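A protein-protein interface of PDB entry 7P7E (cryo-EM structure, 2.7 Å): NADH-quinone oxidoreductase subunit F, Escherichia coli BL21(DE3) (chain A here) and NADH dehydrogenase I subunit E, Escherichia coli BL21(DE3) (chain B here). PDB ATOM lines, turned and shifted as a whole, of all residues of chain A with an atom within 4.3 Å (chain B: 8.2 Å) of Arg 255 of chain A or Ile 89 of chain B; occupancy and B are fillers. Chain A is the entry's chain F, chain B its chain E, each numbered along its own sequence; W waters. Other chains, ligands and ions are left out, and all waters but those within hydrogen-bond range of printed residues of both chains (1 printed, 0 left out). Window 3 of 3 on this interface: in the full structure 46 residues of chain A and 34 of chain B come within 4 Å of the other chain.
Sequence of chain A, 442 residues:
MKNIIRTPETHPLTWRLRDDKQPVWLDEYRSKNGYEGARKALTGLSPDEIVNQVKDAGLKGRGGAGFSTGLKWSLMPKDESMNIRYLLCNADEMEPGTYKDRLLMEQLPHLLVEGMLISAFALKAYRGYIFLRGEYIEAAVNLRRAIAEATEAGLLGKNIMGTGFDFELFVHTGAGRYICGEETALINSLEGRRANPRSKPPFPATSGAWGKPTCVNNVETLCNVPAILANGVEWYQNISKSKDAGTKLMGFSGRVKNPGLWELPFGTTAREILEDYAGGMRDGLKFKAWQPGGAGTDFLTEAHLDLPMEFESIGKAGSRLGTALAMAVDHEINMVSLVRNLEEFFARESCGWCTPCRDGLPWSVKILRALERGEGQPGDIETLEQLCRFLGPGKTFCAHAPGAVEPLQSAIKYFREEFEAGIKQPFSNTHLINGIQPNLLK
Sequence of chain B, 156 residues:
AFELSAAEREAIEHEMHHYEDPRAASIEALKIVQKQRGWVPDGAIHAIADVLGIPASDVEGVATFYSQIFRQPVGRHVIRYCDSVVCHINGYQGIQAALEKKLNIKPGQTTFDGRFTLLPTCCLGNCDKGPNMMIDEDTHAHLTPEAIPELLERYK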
ATOM      1  N   GLY A 254      29.483  17.631  11.124  1.00  0.00           N
ATOM      2  CA  GLY A 254      30.203  17.767   9.876  1.00  0.00           C
ATOM      3  C   GLY A 254      31.163  16.617   9.658  1.00  0.00           C
ATOM      4  O   GLY A 254      30.908  15.499  10.110  1.00  0.00           O
ATOM      5  N   ARG A 255      32.272  16.878   8.972  1.00  0.00           N
ATOM      6  CA  ARG A 255      33.284  15.851   8.729  1.00  0.00           C
ATOM      7  C   ARG A 255      34.376  15.914   9.796  1.00  0.00           C
ATOM      8  O   ARG A 255      35.561  16.092   9.518  1.00  0.00           O
ATOM      9  CB  ARG A 255      33.860  15.998   7.327  1.00  0.00           C
ATOM     10  CG  ARG A 255      32.811  16.082   6.239  1.00  0.00           C
ATOM     11  CD  ARG A 255      32.980  14.975   5.218  1.00  0.00           C
ATOM     12  NE  ARG A 255      33.977  15.314   4.211  1.00  0.00           N
ATOM     13  CZ  ARG A 255      33.695  15.839   3.026  1.00  0.00           C
ATOM     14  NH1 ARG A 255      32.449  16.097   2.665  1.00  0.00           N
ATOM     15  NH2 ARG A 255      34.687  16.112   2.185  1.00  0.00           N
ATOM     16  N   VAL A 256      33.946  15.768  11.042  1.00  0.00           N
ATOM     17  CA  VAL A 256      34.848  15.699  12.169  1.00  0.00           C
ATOM     18  C   VAL A 256      35.004  14.239  12.577  1.00  0.00           C
ATOM     19  O   VAL A 256      34.269  13.364  12.129  1.00  0.00           O
ATOM     20  CB  VAL A 256      34.363  16.573  13.349  1.00  0.00           C
ATOM     21  CG1 VAL A 256      34.328  18.032  12.942  1.00  0.00           C
ATOM     22  CG2 VAL A 256      32.997  16.122  13.814  1.00  0.00           C
ATOM     23  N   MET A 281      39.131  17.582  12.729  1.00  0.00           N
ATOM     24  CA  MET A 281      38.633  17.184  11.423  1.00  0.00           C
ATOM     25  C   MET A 281      39.117  15.781  11.073  1.00  0.00           C
ATOM     26  O   MET A 281      40.035  15.237  11.691  1.00  0.00           O
ATOM     27  CB  MET A 281      39.076  18.177  10.350  1.00  0.00           C
ATOM     28  CG  MET A 281      38.746  19.623  10.669  1.00  0.00           C
ATOM     29  SD  MET A 281      37.005  20.016  10.429  1.00  0.00           S
ATOM     30  CE  MET A 281      36.681  19.213   8.864  1.00  0.00           C
ATOM     31  N   ARG A 282      38.480  15.195  10.064  1.00  0.00           N
ATOM     32  CA  ARG A 282      38.860  13.869   9.613  1.00  0.00           C
ATOM     33  C   ARG A 282      40.192  13.925   8.865  1.00  0.00           C
ATOM     34  O   ARG A 282      40.731  14.996   8.571  1.00  0.00           O
ATOM     35  CB  ARG A 282      37.769  13.270   8.728  1.00  0.00           C
ATOM     36  CG  ARG A 282      36.624  12.648   9.503  1.00  0.00           C
ATOM     37  CD  ARG A 282      35.926  11.575   8.692  1.00  0.00           C
ATOM     38  NE  ARG A 282      34.525  11.897   8.450  1.00  0.00           N
ATOM     39  CZ  ARG A 282      33.940  11.851   7.261  1.00  0.00           C
ATOM     40  NH1 ARG A 282      34.609  11.504   6.175  1.00  0.00           N
ATOM     41  NH2 ARG A 282      32.651  12.161   7.161  1.00  0.00           N
ATOM     42  N   LEU A 285      41.404  16.266   5.607  1.00  0.00           N
ATOM     43  CA  LEU A 285      40.500  17.400   5.483  1.00  0.00           C
ATOM     44  C   LEU A 285      41.009  18.559   6.324  1.00  0.00           C
ATOM     45  O   LEU A 285      41.411  18.371   7.477  1.00  0.00           O
ATOM     46  CB  LEU A 285      39.084  17.018   5.918  1.00  0.00           C
ATOM     47  CG  LEU A 285      38.446  15.896   5.103  1.00  0.00           C
ATOM     48  CD1 LEU A 285      37.138  15.459   5.722  1.00  0.00           C
ATOM     49  CD2 LEU A 285      38.239  16.341   3.670  1.00  0.00           C
ATOM     50  N   MET A 327      28.784  23.533  13.309  1.00  0.00           N
ATOM     51  CA  MET A 327      28.972  22.696  12.135  1.00  0.00           C
ATOM     52  C   MET A 327      30.253  23.122  11.438  1.00  0.00           C
ATOM     53  O   MET A 327      30.463  24.316  11.205  1.00  0.00           O
ATOM     54  CB  MET A 327      27.780  22.814  11.186  1.00  0.00           C
ATOM     55  CG  MET A 327      27.959  22.108   9.865  1.00  0.00           C
ATOM     56  SD  MET A 327      26.732  22.666   8.679  1.00  0.00           S
ATOM     57  CE  MET A 327      27.565  24.102   8.013  1.00  0.00           C
ATOM     58  N   ALA A 328      31.100  22.151  11.107  1.00  0.00           N
ATOM     59  CA  ALA A 328      32.398  22.408  10.502  1.00  0.00           C
ATOM     60  C   ALA A 328      32.331  22.222   8.992  1.00  0.00           C
ATOM     61  O   ALA A 328      31.710  21.278   8.498  1.00  0.00           O
ATOM     62  CB  ALA A 328      33.465  21.487  11.092  1.00  0.00           C
ATOM     63  N   VAL A 329      32.976  23.131   8.267  1.00  0.00           N
ATOM     64  CA  VAL A 329      33.044  23.116   6.813  1.00  0.00           C
ATOM     65  C   VAL A 329      34.509  22.980   6.428  1.00  0.00           C
ATOM     66  O   VAL A 329      35.333  23.830   6.796  1.00  0.00           O
ATOM     67  CB  VAL A 329      32.438  24.388   6.201  1.00  0.00           C
ATOM     68  CG1 VAL A 329      32.374  24.273   4.690  1.00  0.00           C
ATOM     69  CG2 VAL A 329      31.064  24.661   6.784  1.00  0.00           C
ATOM     70  N   ASP A 330      34.826  21.923   5.681  1.00  0.00           N
ATOM     71  CA  ASP A 330      36.183  21.634   5.251  1.00  0.00           C
ATOM     72  C   ASP A 330      36.444  22.227   3.868  1.00  0.00           C
ATOM     73  O   ASP A 330      35.550  22.771   3.217  1.00  0.00           O
ATOM     74  CB  ASP A 330      36.434  20.128   5.251  1.00  0.00           C
ATOM     75  CG  ASP A 330      35.262  19.341   4.706  1.00  0.00           C
ATOM     76  OD1 ASP A 330      34.108  19.754   4.938  1.00  0.00           O
ATOM     77  OD2 ASP A 330      35.493  18.313   4.040  1.00  0.00           O
ATOM     78  N   GLU A 332      37.009  20.862   1.010  1.00  0.00           N
ATOM     79  CA  GLU A 332      36.396  20.217  -0.144  1.00  0.00           C
ATOM     80  C   GLU A 332      34.998  20.737  -0.446  1.00  0.00           C
ATOM     81  O   GLU A 332      34.443  20.397  -1.496  1.00  0.00           O
ATOM     82  CB  GLU A 332      36.341  18.703   0.065  1.00  0.00           C
ATOM     83  CG  GLU A 332      37.696  18.020   0.016  1.00  0.00           C
ATOM     84  CD  GLU A 332      37.594  16.516   0.168  1.00  0.00           C
ATOM     85  OE1 GLU A 332      36.470  16.014   0.384  1.00  0.00           O
ATOM     86  OE2 GLU A 332      38.636  15.834   0.073  1.00  0.00           O
ATOM     87  N   ILE A 333      34.419  21.548   0.432  1.00  0.00           N
ATOM     88  CA  ILE A 333      33.060  22.042   0.258  1.00  0.00           C
ATOM     89  C   ILE A 333      33.112  23.391  -0.447  1.00  0.00           C
ATOM     90  O   ILE A 333      33.770  24.325   0.022  1.00  0.00           O
ATOM     91  CB  ILE A 333      32.333  22.154   1.606  1.00  0.00           C
ATOM     92  CG1 ILE A 333      32.272  20.788   2.291  1.00  0.00           C
ATOM     93  CG2 ILE A 333      30.937  22.716   1.414  1.00  0.00           C
ATOM     94  CD1 ILE A 333      31.545  19.738   1.488  1.00  0.00           C
ATOM     95  N   LEU A 338      27.208  25.358  -0.723  1.00  0.00           N
ATOM     96  CA  LEU A 338      26.686  25.256   0.636  1.00  0.00           C
ATOM     97  C   LEU A 338      25.659  26.345   0.919  1.00  0.00           C
ATOM     98  O   LEU A 338      24.584  26.077   1.473  1.00  0.00           O
ATOM     99  CB  LEU A 338      27.837  25.336   1.634  1.00  0.00           C
ATOM    100  CG  LEU A 338      27.545  24.794   3.027  1.00  0.00           C
ATOM    101  CD1 LEU A 338      27.398  23.296   2.950  1.00  0.00           C
ATOM    102  CD2 LEU A 338      28.649  25.184   3.986  1.00  0.00           C
ATOM    103  N   ASP B  83      17.973  16.734   2.698  1.00  0.00           N
ATOM    104  CA  ASP B  83      18.766  17.521   1.763  1.00  0.00           C
ATOM    105  C   ASP B  83      19.299  18.800   2.400  1.00  0.00           C
ATOM    106  O   ASP B  83      19.617  19.757   1.690  1.00  0.00           O
ATOM    107  CB  ASP B  83      17.962  17.837   0.494  1.00  0.00           C
ATOM    108  CG  ASP B  83      16.757  18.738   0.738  1.00  0.00           C
ATOM    109  OD1 ASP B  83      16.371  18.983   1.896  1.00  0.00           O
ATOM    110  OD2 ASP B  83      16.178  19.208  -0.262  1.00  0.00           O
ATOM    111  N   SER B  84      19.402  18.834   3.724  1.00  0.00           N
ATOM    112  CA  SER B  84      19.817  20.033   4.429  1.00  0.00           C
ATOM    113  C   SER B  84      21.343  20.106   4.475  1.00  0.00           C
ATOM    114  O   SER B  84      22.045  19.317   3.838  1.00  0.00           O
ATOM    115  CB  SER B  84      19.185  20.074   5.816  1.00  0.00           C
ATOM    116  OG  SER B  84      17.839  20.504   5.741  1.00  0.00           O
ATOM    117  N   VAL B  85      21.867  21.056   5.250  1.00  0.00           N
ATOM    118  CA  VAL B  85      23.242  21.510   5.061  1.00  0.00           C
ATOM    119  C   VAL B  85      24.250  20.490   5.592  1.00  0.00           C
ATOM    120  O   VAL B  85      25.266  20.215   4.940  1.00  0.00           O
ATOM    121  CB  VAL B  85      23.419  22.908   5.691  1.00  0.00           C
ATOM    122  CG1 VAL B  85      22.884  22.961   7.122  1.00  0.00           C
ATOM    123  CG2 VAL B  85      24.854  23.366   5.616  1.00  0.00           C
ATOM    124  N   VAL B  86      23.992  19.906   6.765  1.00  0.00           N
ATOM    125  CA  VAL B  86      24.945  18.961   7.343  1.00  0.00           C
ATOM    126  C   VAL B  86      24.982  17.674   6.530  1.00  0.00           C
ATOM    127  O   VAL B  86      26.050  17.084   6.326  1.00  0.00           O
ATOM    128  CB  VAL B  86      24.616  18.688   8.821  1.00  0.00           C
ATOM    129  CG1 VAL B  86      25.799  18.034   9.511  1.00  0.00           C
ATOM    130  CG2 VAL B  86      24.235  19.974   9.524  1.00  0.00           C
ATOM    131  N   CYS B  87      23.827  17.223   6.043  1.00  0.00           N
ATOM    132  CA  CYS B  87      23.806  16.065   5.161  1.00  0.00           C
ATOM    133  C   CYS B  87      24.352  16.390   3.777  1.00  0.00           C
ATOM    134  O   CYS B  87      24.811  15.482   3.078  1.00  0.00           O
ATOM    135  CB  CYS B  87      22.387  15.509   5.060  1.00  0.00           C
ATOM    136  SG  CYS B  87      21.794  14.776   6.598  1.00  0.00           S
ATOM    137  N   HIS B  88      24.303  17.659   3.364  1.00  0.00           N
ATOM    138  CA  HIS B  88      24.999  18.070   2.149  1.00  0.00           C
ATOM    139  C   HIS B  88      26.507  17.979   2.328  1.00  0.00           C
ATOM    140  O   HIS B  88      27.226  17.595   1.400  1.00  0.00           O
ATOM    141  CB  HIS B  88      24.586  19.490   1.759  1.00  0.00           C
ATOM    142  CG  HIS B  88      25.363  20.052   0.611  1.00  0.00           C
ATOM    143  ND1 HIS B  88      25.003  19.847  -0.702  1.00  0.00           N
ATOM    144  CD2 HIS B  88      26.480  20.818   0.579  1.00  0.00           C
ATOM    145  CE1 HIS B  88      25.864  20.458  -1.494  1.00  0.00           C
ATOM    146  NE2 HIS B  88      26.771  21.054  -0.741  1.00  0.00           N
ATOM    147  N   ILE B  89      26.999  18.343   3.512  1.00  0.00           N
ATOM    148  CA  ILE B  89      28.418  18.187   3.815  1.00  0.00           C
ATOM    149  C   ILE B  89      28.789  16.710   3.881  1.00  0.00           C
ATOM    150  O   ILE B  89      29.840  16.293   3.380  1.00  0.00           O
ATOM    151  CB  ILE B  89      28.755  18.934   5.119  1.00  0.00           C
ATOM    152  CG1 ILE B  89      28.685  20.443   4.887  1.00  0.00           C
ATOM    153  CG2 ILE B  89      30.125  18.548   5.642  1.00  0.00           C
ATOM    154  CD1 ILE B  89      29.081  21.269   6.083  1.00  0.00           C
ATOM    155  N   ASN B  90      27.912  15.890   4.456  1.00  0.00           N
ATOM    156  CA  ASN B  90      28.162  14.461   4.600  1.00  0.00           C
ATOM    157  C   ASN B  90      27.854  13.666   3.338  1.00  0.00           C
ATOM    158  O   ASN B  90      28.021  12.443   3.344  1.00  0.00           O
ATOM    159  CB  ASN B  90      27.352  13.906   5.773  1.00  0.00           C
ATOM    160  CG  ASN B  90      27.914  14.320   7.114  1.00  0.00           C
ATOM    161  OD1 ASN B  90      29.127  14.328   7.313  1.00  0.00           O
ATOM    162  ND2 ASN B  90      27.035  14.670   8.042  1.00  0.00           N
ATOM    163  N   GLY B  91      27.406  14.317   2.268  1.00  0.00           N
ATOM    164  CA  GLY B  91      27.242  13.647   0.995  1.00  0.00           C
ATOM    165  C   GLY B  91      25.891  13.006   0.758  1.00  0.00           C
ATOM    166  O   GLY B  91      25.815  11.809   0.468  1.00  0.00           O
ATOM    167  N   TYR B  92      24.813  13.785   0.874  1.00  0.00           N
ATOM    168  CA  TYR B  92      23.492  13.251   0.565  1.00  0.00           C
ATOM    169  C   TYR B  92      23.273  13.088  -0.933  1.00  0.00           C
ATOM    170  O   TYR B  92      22.361  12.357  -1.327  1.00  0.00           O
ATOM    171  CB  TYR B  92      22.391  14.142   1.160  1.00  0.00           C
ATOM    172  CG  TYR B  92      21.883  15.243   0.242  1.00  0.00           C
ATOM    173  CD1 TYR B  92      22.525  16.470   0.189  1.00  0.00           C
ATOM    174  CD2 TYR B  92      20.747  15.066  -0.548  1.00  0.00           C
ATOM    175  CE1 TYR B  92      22.075  17.478  -0.635  1.00  0.00           C
ATOM    176  CE2 TYR B  92      20.302  16.063  -1.385  1.00  0.00           C
ATOM    177  CZ  TYR B  92      20.962  17.271  -1.417  1.00  0.00           C
ATOM    178  OH  TYR B  92      20.512  18.277  -2.239  1.00  0.00           O
ATOM    179  N   GLN B  93      24.054  13.778  -1.769  1.00  0.00           N
ATOM    180  CA  GLN B  93      23.823  13.717  -3.209  1.00  0.00           C
ATOM    181  C   GLN B  93      24.147  12.346  -3.780  1.00  0.00           C
ATOM    182  O   GLN B  93      23.488  11.905  -4.726  1.00  0.00           O
ATOM    183  CB  GLN B  93      24.627  14.800  -3.927  1.00  0.00           C
ATOM    184  CG  GLN B  93      23.936  16.154  -3.958  1.00  0.00           C
ATOM    185  CD  GLN B  93      24.771  17.254  -3.341  1.00  0.00           C
ATOM    186  OE1 GLN B  93      25.351  17.082  -2.272  1.00  0.00           O
ATOM    187  NE2 GLN B  93      24.835  18.396  -4.014  1.00  0.00           N
ATOM    188  N   CYS B 127      21.854  15.074  12.656  1.00  0.00           N
ATOM    189  CA  CYS B 127      22.921  15.590  11.803  1.00  0.00           C
ATOM    190  C   CYS B 127      24.276  14.983  12.134  1.00  0.00           C
ATOM    191  O   CYS B 127      25.136  14.882  11.252  1.00  0.00           O
ATOM    192  CB  CYS B 127      22.981  17.109  11.919  1.00  0.00           C
ATOM    193  SG  CYS B 127      21.360  17.874  11.973  1.00  0.00           S
ATOM    194  N   GLY B 130      24.731  11.755  10.003  1.00  0.00           N
ATOM    195  CA  GLY B 130      24.335  11.939   8.628  1.00  0.00           C
ATOM    196  C   GLY B 130      25.173  11.145   7.645  1.00  0.00           C
ATOM    197  O   GLY B 130      26.267  10.676   7.971  1.00  0.00           O
ATOM    198  N   PRO B 131      24.676  10.976   6.407  1.00  0.00           N
ATOM    199  CA  PRO B 131      23.381  11.443   5.892  1.00  0.00           C
ATOM    200  C   PRO B 131      22.209  10.585   6.361  1.00  0.00           C
ATOM    201  O   PRO B 131      22.401   9.421   6.699  1.00  0.00           O
ATOM    202  CB  PRO B 131      23.554  11.349   4.376  1.00  0.00           C
ATOM    203  CG  PRO B 131      24.556  10.284   4.182  1.00  0.00           C
ATOM    204  CD  PRO B 131      25.486  10.340   5.354  1.00  0.00           C
HETATM  205  O   HOH W   1      28.184  15.122  11.036  1.00  0.00           O
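NH1 of Arg 255 of chain A sits at hydrogen-bond distance from O of Ile 89 of chain B, 2.7 Å away.
The side-chain amide oxygen of Gln 93 of chain B lies within hydrogen-bond range of a ring nitrogen (ND1) of His 88 of chain B. The side-chain carboxylate of Asp 330 of chain A lies within salt-bridge range of the guanidinium group of Arg 255 of chain A (3.0 Å). The backbone NH (N) of Arg 282 of chain A sits at hydrogen-bond distance from the backbone carbonyl oxygen (O) of Arg 255 of chain A. OE1 of Glu 332 of chain A lies within salt-bridge range of NH2 of Arg 255 of chain A, at 2.5 Å. O of Val 86 of chain B sits at hydrogen-bond distance from ND2 of Asn 90 of chain B.
Asn 90 of chain B touches Gly 254 of chain A. Val 85 of chain B touches Met 327 of chain A. Val 86 of chain B touches Met 327 of chain A. Ile 89 of chain B touches Met 327 of chain A. Ile 89 of chain B touches Ala 328 of chain A. Val 329 of chain A touches Ile 89 of chain B (CG2 to CD1, 3.99 Å). CD1 of Leu 338 of chain A touches CG2 of Val 85 of chain B, at 3.7 Å. His 88 of chain B touches Leu 338 of chain A. CD1 of Leu 338 of chain A touches CG1 of Ile 89 of chain B, at 3.7 Å.
Arg 255 of chain A touches just one residue of chain B: Ile 89. Of the printed residues of chain B, Met 327 of chain A touches Val 85 (3.7 Å), Val 86 (3.8 Å) and Ile 89 (3.7 Å). Of the printed residues of chain B, Ala 328 of chain A touches Ile 89 (3.6 Å). Of the printed residues of chain B, Leu 338 of chain A touches Val 85 (3.7 Å), His 88 (3.6 Å) and Ile 89 (3.7 Å). Of the printed residues of chain A, His 88 of chain B touches Leu 338. Printed residues of chain A within 4 Å of Ile 89 of chain B: Arg 255, Met 327, Ala 328, Val 329 and Leu 338. Of the printed residues of chain A, Asn 90 of chain B touches Gly 254.
Along chain A the printed residues that touch a printed residue of chain B span positions 254 to 338. Of the 14 printed residues of chain B, 5 touch a printed residue of chain A. Hydrophobic or aromatic side chains of chain B that line the printed part of chain A: Val 85, Val 86, His 88 and Ile 89. Among the printed residues, 10 pairs touch across the chains. Among the printed residues, no Asp or Glu carboxylate lies within 4 Å of a Lys or Arg side-chain nitrogen of the other chain.
Water W1 lies within hydrogen-bond range of N of Gly 254 of chain A (2.8 Å), O of Cys 127 of chain B (3.1 Å) and ND2 of Asn 90 of chain B (3.2 Å).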
